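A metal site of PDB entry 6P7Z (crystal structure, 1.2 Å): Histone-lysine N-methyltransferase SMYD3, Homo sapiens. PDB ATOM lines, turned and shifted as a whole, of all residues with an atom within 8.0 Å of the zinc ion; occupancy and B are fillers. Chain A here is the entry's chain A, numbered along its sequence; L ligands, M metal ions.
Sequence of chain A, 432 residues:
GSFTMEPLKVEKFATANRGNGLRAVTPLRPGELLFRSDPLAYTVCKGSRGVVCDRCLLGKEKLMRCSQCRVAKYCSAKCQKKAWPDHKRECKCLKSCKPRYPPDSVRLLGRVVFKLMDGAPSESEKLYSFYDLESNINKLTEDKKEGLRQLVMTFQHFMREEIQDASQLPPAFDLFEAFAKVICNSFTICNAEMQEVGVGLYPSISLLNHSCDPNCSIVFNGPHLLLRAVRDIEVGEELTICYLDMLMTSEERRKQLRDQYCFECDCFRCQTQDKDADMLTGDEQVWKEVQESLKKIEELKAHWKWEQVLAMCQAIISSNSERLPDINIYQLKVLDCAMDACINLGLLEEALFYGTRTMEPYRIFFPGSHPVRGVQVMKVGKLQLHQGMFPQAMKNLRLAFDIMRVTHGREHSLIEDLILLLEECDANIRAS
N of Cys 212 is in hydrogen-bond range of NE2 of His 210, at 3.4 Å.
The side-chain sulfur (SG) of Cys 212 sits close to the guanidinium group (NE) of Arg 253 (3.2 Å).
N of Arg 269 lies close to SG of Cys 267 (3.5 Å).
O of Cys 212 is in hydrogen-bond range of NH1 of Arg 269 (3.1 Å).
The side-chain sulfur of Cys 270 sits close to the guanidinium group of Arg 253 (3.4 Å).
A nitrogen (N4) of the ligand sits at hydrogen-bond distance from the backbone carbonyl oxygen (O) of His 210.
The backbone NH of His 210 lies within hydrogen-bond range of a nitrogen (N3) of the ligand (2.9 Å).
The zinc ion is bound by the side-chain sulfur (SG) of Cys 267 (2.3 Å).
The zinc ion is bound by SG of Cys 265, 2.3 Å away.
SG of Cys 270 binds the zinc ion, 2.3 Å away.
SG of Cys 212 is bound to the zinc ion, at 2.3 Å.
The zinc ion has four donor atoms within binding distance.
Within 4 Å of the zinc ion: Cys 212, Cys 265, Cys 267 and Cys 270.
The nearest printed residue that does not touch the zinc ion is Arg 253 (4.5 Å).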
ATOM      1  N   HIS A 210     -25.936  13.271  35.621  1.00  0.00           N
ATOM      2  CA  HIS A 210     -25.699  12.043  34.892  1.00  0.00           C
ATOM      3  C   HIS A 210     -24.225  11.695  34.822  1.00  0.00           C
ATOM      4  O   HIS A 210     -23.363  12.583  34.661  1.00  0.00           O
ATOM      5  CB  HIS A 210     -26.203  12.215  33.453  1.00  0.00           C
ATOM      6  CG  HIS A 210     -25.699  11.173  32.525  1.00  0.00           C
ATOM      7  ND1 HIS A 210     -26.299   9.940  32.372  1.00  0.00           N
ATOM      8  CD2 HIS A 210     -24.598  11.158  31.723  1.00  0.00           C
ATOM      9  CE1 HIS A 210     -25.611   9.228  31.497  1.00  0.00           C
ATOM     10  NE2 HIS A 210     -24.563   9.935  31.110  1.00  0.00           N
ATOM     11  N   SER A 211     -23.938  10.403  34.877  1.00  0.00           N
ATOM     12  CA  SER A 211     -22.647   9.869  34.479  1.00  0.00           C
ATOM     13  C   SER A 211     -22.855   8.569  33.734  1.00  0.00           C
ATOM     14  O   SER A 211     -23.747   7.782  34.085  1.00  0.00           O
ATOM     15  CB  SER A 211     -21.763   9.616  35.702  1.00  0.00           C
ATOM     16  OG  SER A 211     -20.598   8.913  35.294  1.00  0.00           O
ATOM     17  N   CYS A 212     -22.024   8.319  32.718  1.00  0.00           N
ATOM     18  CA  CYS A 212     -22.015   7.048  32.014  1.00  0.00           C
ATOM     19  C   CYS A 212     -21.317   5.937  32.809  1.00  0.00           C
ATOM     20  O   CYS A 212     -21.300   4.789  32.362  1.00  0.00           O
ATOM     21  CB  CYS A 212     -21.373   7.191  30.627  1.00  0.00           C
ATOM     22  SG  CYS A 212     -22.017   8.528  29.616  1.00  0.00           S
ATOM     23  N   ASP A 213     -20.783   6.288  33.984  1.00  0.00           N
ATOM     24  CA  ASP A 213     -20.200   5.332  34.922  1.00  0.00           C
ATOM     25  C   ASP A 213     -20.466   5.867  36.324  1.00  0.00           C
ATOM     26  O   ASP A 213     -19.596   6.462  36.957  1.00  0.00           O
ATOM     27  CB  ASP A 213     -18.699   5.156  34.672  1.00  0.00           C
ATOM     28  CG  ASP A 213     -18.062   4.152  35.613  1.00  0.00           C
ATOM     29  OD1 ASP A 213     -18.782   3.443  36.352  1.00  0.00           O
ATOM     30  OD2 ASP A 213     -16.819   4.052  35.605  1.00  0.00           O
ATOM     31  N   CYS A 242     -26.783   7.062  36.084  1.00  0.00           N
ATOM     32  CA  CYS A 242     -26.797   7.000  34.629  1.00  0.00           C
ATOM     33  C   CYS A 242     -28.232   7.169  34.147  1.00  0.00           C
ATOM     34  O   CYS A 242     -29.090   6.346  34.467  1.00  0.00           O
ATOM     35  CB  CYS A 242     -26.185   5.699  34.137  1.00  0.00           C
ATOM     36  SG  CYS A 242     -25.987   5.662  32.330  1.00  0.00           S
ATOM     37  N   LEU A 244     -29.316   6.710  31.276  1.00  0.00           N
ATOM     38  CA  LEU A 244     -29.547   5.981  30.035  1.00  0.00           C
ATOM     39  C   LEU A 244     -29.365   4.482  30.205  1.00  0.00           C
ATOM     40  O   LEU A 244     -28.601   4.016  31.057  1.00  0.00           O
ATOM     41  CB  LEU A 244     -28.554   6.439  28.978  1.00  0.00           C
ATOM     42  CG  LEU A 244     -28.503   7.927  28.704  1.00  0.00           C
ATOM     43  CD1 LEU A 244     -27.465   8.209  27.634  1.00  0.00           C
ATOM     44  CD2 LEU A 244     -29.862   8.382  28.251  1.00  0.00           C
ATOM     45  N   SER A 250     -21.434   5.277  22.510  1.00  0.00           N
ATOM     46  CA  SER A 250     -21.211   6.679  22.865  1.00  0.00           C
ATOM     47  C   SER A 250     -21.905   7.641  21.902  1.00  0.00           C
ATOM     48  O   SER A 250     -22.338   8.716  22.315  1.00  0.00           O
ATOM     49  CB  SER A 250     -19.724   7.006  22.977  1.00  0.00           C
ATOM     50  OG  SER A 250     -19.061   6.869  21.739  1.00  0.00           O
ATOM     51  N   ARG A 253     -25.534   7.615  23.034  1.00  0.00           N
ATOM     52  CA  ARG A 253     -25.641   8.433  24.241  1.00  0.00           C
ATOM     53  C   ARG A 253     -25.528   9.908  23.899  1.00  0.00           C
ATOM     54  O   ARG A 253     -26.282  10.720  24.435  1.00  0.00           O
ATOM     55  CB  ARG A 253     -24.582   8.028  25.272  1.00  0.00           C
ATOM     56  CG  ARG A 253     -24.697   6.579  25.710  1.00  0.00           C
ATOM     57  CD  ARG A 253     -23.973   6.311  27.036  1.00  0.00           C
ATOM     58  NE  ARG A 253     -22.557   6.667  27.013  1.00  0.00           N
ATOM     59  CZ  ARG A 253     -21.587   5.903  26.512  1.00  0.00           C
ATOM     60  NH1 ARG A 253     -21.877   4.722  25.961  1.00  0.00           N
ATOM     61  NH2 ARG A 253     -20.339   6.337  26.557  1.00  0.00           N
ATOM     62  N   ARG A 254     -24.618  10.270  23.011  1.00  0.00           N
ATOM     63  CA  ARG A 254     -24.471  11.682  22.657  1.00  0.00           C
ATOM     64  C   ARG A 254     -25.776  12.232  22.118  1.00  0.00           C
ATOM     65  O   ARG A 254     -26.211  13.337  22.491  1.00  0.00           O
ATOM     66  CB  ARG A 254     -23.353  11.857  21.628  1.00  0.00           C
ATOM     67  CG  ARG A 254     -23.294  13.272  21.042  1.00  0.00           C
ATOM     68  CD  ARG A 254     -22.051  13.479  20.174  1.00  0.00           C
ATOM     69  NE  ARG A 254     -20.841  13.336  20.974  1.00  0.00           N
ATOM     70  CZ  ARG A 254     -19.994  12.316  20.911  1.00  0.00           C
ATOM     71  NH1 ARG A 254     -20.188  11.337  20.039  1.00  0.00           N
ATOM     72  NH2 ARG A 254     -18.953  12.276  21.719  1.00  0.00           N
ATOM     73  N   LEU A 257     -28.417  12.470  25.041  1.00  0.00           N
ATOM     74  CA  LEU A 257     -28.078  13.509  26.015  1.00  0.00           C
ATOM     75  C   LEU A 257     -28.219  14.908  25.428  1.00  0.00           C
ATOM     76  O   LEU A 257     -28.642  15.833  26.130  1.00  0.00           O
ATOM     77  CB  LEU A 257     -26.689  13.269  26.598  1.00  0.00           C
ATOM     78  CG  LEU A 257     -26.536  11.955  27.380  1.00  0.00           C
ATOM     79  CD1 LEU A 257     -25.100  11.775  27.823  1.00  0.00           C
ATOM     80  CD2 LEU A 257     -27.483  11.881  28.573  1.00  0.00           C
ATOM     81  N   PHE A 263     -27.060  18.484  26.967  1.00  0.00           N
ATOM     82  CA  PHE A 263     -25.660  18.621  27.366  1.00  0.00           C
ATOM     83  C   PHE A 263     -24.782  17.661  26.593  1.00  0.00           C
ATOM     84  O   PHE A 263     -25.250  16.700  25.988  1.00  0.00           O
ATOM     85  CB  PHE A 263     -25.411  18.509  28.874  1.00  0.00           C
ATOM     86  CG  PHE A 263     -25.531  17.110  29.423  1.00  0.00           C
ATOM     87  CD1 PHE A 263     -26.767  16.610  29.821  1.00  0.00           C
ATOM     88  CD2 PHE A 263     -24.411  16.292  29.562  1.00  0.00           C
ATOM     89  CE1 PHE A 263     -26.877  15.331  30.347  1.00  0.00           C
ATOM     90  CE2 PHE A 263     -24.520  15.003  30.091  1.00  0.00           C
ATOM     91  CZ  PHE A 263     -25.758  14.529  30.472  1.00  0.00           C
ATOM     92  N   GLU A 264     -23.473  17.968  26.612  1.00  0.00           N
ATOM     93  CA  GLU A 264     -22.411  17.189  25.993  1.00  0.00           C
ATOM     94  C   GLU A 264     -21.630  16.503  27.102  1.00  0.00           C
ATOM     95  O   GLU A 264     -21.180  17.159  28.048  1.00  0.00           O
ATOM     96  CB  GLU A 264     -21.448  18.120  25.233  1.00  0.00           C
ATOM     97  CG  GLU A 264     -22.118  19.263  24.471  1.00  0.00           C
ATOM     98  CD  GLU A 264     -22.962  18.775  23.303  1.00  0.00           C
ATOM     99  OE1 GLU A 264     -23.727  19.590  22.740  1.00  0.00           O
ATOM    100  OE2 GLU A 264     -22.871  17.580  22.932  1.00  0.00           O
ATOM    101  N   CYS A 265     -21.511  15.185  27.035  1.00  0.00           N
ATOM    102  CA  CYS A 265     -20.906  14.428  28.127  1.00  0.00           C
ATOM    103  C   CYS A 265     -19.403  14.353  27.943  1.00  0.00           C
ATOM    104  O   CYS A 265     -18.918  13.927  26.881  1.00  0.00           O
ATOM    105  CB  CYS A 265     -21.452  13.005  28.254  1.00  0.00           C
ATOM    106  SG  CYS A 265     -21.023  12.152  29.812  1.00  0.00           S
ATOM    107  N   ASP A 266     -18.671  14.747  28.988  1.00  0.00           N
ATOM    108  CA  ASP A 266     -17.223  14.827  29.010  1.00  0.00           C
ATOM    109  C   ASP A 266     -16.558  13.637  29.712  1.00  0.00           C
ATOM    110  O   ASP A 266     -15.347  13.655  29.919  1.00  0.00           O
ATOM    111  CB  ASP A 266     -16.764  16.140  29.655  1.00  0.00           C
ATOM    112  CG  ASP A 266     -17.114  16.235  31.142  1.00  0.00           C
ATOM    113  OD1 ASP A 266     -17.892  15.397  31.654  1.00  0.00           O
ATOM    114  OD2 ASP A 266     -16.593  17.157  31.821  1.00  0.00           O
ATOM    115  N   CYS A 267     -17.329  12.607  30.090  1.00  0.00           N
ATOM    116  CA  CYS A 267     -16.796  11.532  30.913  1.00  0.00           C
ATOM    117  C   CYS A 267     -15.748  10.700  30.142  1.00  0.00           C
ATOM    118  O   CYS A 267     -15.605  10.786  28.921  1.00  0.00           O
ATOM    119  CB  CYS A 267     -17.923  10.669  31.473  1.00  0.00           C
ATOM    120  SG  CYS A 267     -18.481   9.380  30.373  1.00  0.00           S
ATOM    121  N   PHE A 268     -14.967   9.920  30.903  1.00  0.00           N
ATOM    122  CA  PHE A 268     -13.913   9.111  30.292  1.00  0.00           C
ATOM    123  C   PHE A 268     -14.469   8.167  29.234  1.00  0.00           C
ATOM    124  O   PHE A 268     -13.850   7.935  28.196  1.00  0.00           O
ATOM    125  CB  PHE A 268     -13.154   8.327  31.354  1.00  0.00           C
ATOM    126  CG  PHE A 268     -12.315   7.205  30.800  1.00  0.00           C
ATOM    127  CD1 PHE A 268     -11.069   7.470  30.258  1.00  0.00           C
ATOM    128  CD2 PHE A 268     -12.780   5.901  30.805  1.00  0.00           C
ATOM    129  CE1 PHE A 268     -10.289   6.458  29.746  1.00  0.00           C
ATOM    130  CE2 PHE A 268     -11.999   4.877  30.285  1.00  0.00           C
ATOM    131  CZ  PHE A 268     -10.754   5.154  29.750  1.00  0.00           C
ATOM    132  N   ARG A 269     -15.648   7.593  29.498  1.00  0.00           N
ATOM    133  CA  ARG A 269     -16.204   6.629  28.560  1.00  0.00           C
ATOM    134  C   ARG A 269     -16.530   7.302  27.230  1.00  0.00           C
ATOM    135  O   ARG A 269     -16.264   6.725  26.170  1.00  0.00           O
ATOM    136  CB  ARG A 269     -17.449   5.971  29.145  1.00  0.00           C
ATOM    137  CG  ARG A 269     -17.187   5.110  30.378  1.00  0.00           C
ATOM    138  CD  ARG A 269     -18.367   4.179  30.666  1.00  0.00           C
ATOM    139  NE  ARG A 269     -18.575   3.284  29.533  1.00  0.00           N
ATOM    140  CZ  ARG A 269     -19.761   2.984  29.008  1.00  0.00           C
ATOM    141  NH1 ARG A 269     -20.887   3.445  29.545  1.00  0.00           N
ATOM    142  NH2 ARG A 269     -19.819   2.202  27.942  1.00  0.00           N
ATOM    143  N   CYS A 270     -17.101   8.505  27.273  1.00  0.00           N
ATOM    144  CA  CYS A 270     -17.429   9.199  26.020  1.00  0.00           C
ATOM    145  C   CYS A 270     -16.175   9.641  25.286  1.00  0.00           C
ATOM    146  O   CYS A 270     -16.086   9.525  24.066  1.00  0.00           O
ATOM    147  CB  CYS A 270     -18.379  10.356  26.313  1.00  0.00           C
ATOM    148  SG  CYS A 270     -19.998   9.729  26.857  1.00  0.00           S
ATOM    149  N   GLN A 271     -15.166  10.110  26.029  1.00  0.00           N
ATOM    150  CA  GLN A 271     -13.934  10.555  25.387  1.00  0.00           C
ATOM    151  C   GLN A 271     -13.212   9.413  24.679  1.00  0.00           C
ATOM    152  O   GLN A 271     -12.531   9.642  23.675  1.00  0.00           O
ATOM    153  CB  GLN A 271     -12.991  11.202  26.422  1.00  0.00           C
ATOM    154  CG  GLN A 271     -13.540  12.443  27.139  1.00  0.00           C
ATOM    155  CD  GLN A 271     -12.586  12.936  28.216  1.00  0.00           C
ATOM    156  OE1 GLN A 271     -11.374  12.981  28.023  1.00  0.00           O
ATOM    157  NE2 GLN A 271     -13.136  13.290  29.379  1.00  0.00           N
HETATM  158  N1  LIG L   1     -28.275  19.991  36.989  1.00  0.00           N
HETATM  159  C1  LIG L   1     -29.728  19.826  37.155  1.00  0.00           C
HETATM  160  C2  LIG L   1     -30.365  21.052  37.801  1.00  0.00           C
HETATM  161  O1  LIG L   1     -31.558  21.011  38.119  1.00  0.00           O
HETATM  162  O2  LIG L   1     -29.646  22.058  37.967  1.00  0.00           O
HETATM  163  C3  LIG L   1     -30.039  18.539  37.906  1.00  0.00           C
HETATM  164  C4  LIG L   1     -30.092  17.318  36.979  1.00  0.00           C
HETATM  165  S1  LIG L   1     -31.535  17.402  35.878  1.00  0.00           S
HETATM  166  C5  LIG L   1     -32.329  15.803  36.118  1.00  0.00           C
HETATM  167  C6  LIG L   1     -30.800  17.158  34.225  1.00  0.00           C
HETATM  168  C7  LIG L   1     -30.030  18.341  33.681  1.00  0.00           C
HETATM  169  O3  LIG L   1     -28.835  18.501  34.420  1.00  0.00           O
HETATM  170  C8  LIG L   1     -29.571  18.144  32.246  1.00  0.00           C
HETATM  171  O4  LIG L   1     -30.623  18.443  31.357  1.00  0.00           O
HETATM  172  C9  LIG L   1     -28.383  19.075  32.187  1.00  0.00           C
HETATM  173  O5  LIG L   1     -28.855  20.421  32.153  1.00  0.00           O
HETATM  174  C10 LIG L   1     -27.772  18.837  33.543  1.00  0.00           C
HETATM  175  N2  LIG L   1     -26.807  17.720  33.582  1.00  0.00           N
HETATM  176  C11 LIG L   1     -27.030  16.466  34.119  1.00  0.00           C
HETATM  177  N3  LIG L   1     -25.914  15.725  34.010  1.00  0.00           N
HETATM  178  C12 LIG L   1     -24.969  16.490  33.408  1.00  0.00           C
HETATM  179  C13 LIG L   1     -23.643  16.265  33.031  1.00  0.00           C
HETATM  180  N4  LIG L   1     -22.988  15.109  33.248  1.00  0.00           N
HETATM  181  N5  LIG L   1     -22.949  17.279  32.427  1.00  0.00           N
HETATM  182  C14 LIG L   1     -23.559  18.493  32.176  1.00  0.00           C
HETATM  183  N6  LIG L   1     -24.857  18.743  32.526  1.00  0.00           N
HETATM  184  C15 LIG L   1     -25.522  17.744  33.137  1.00  0.00           C
HETATM  185 ZN    ZN M   1     -20.293  10.048  29.156  1.00  0.00          ZN
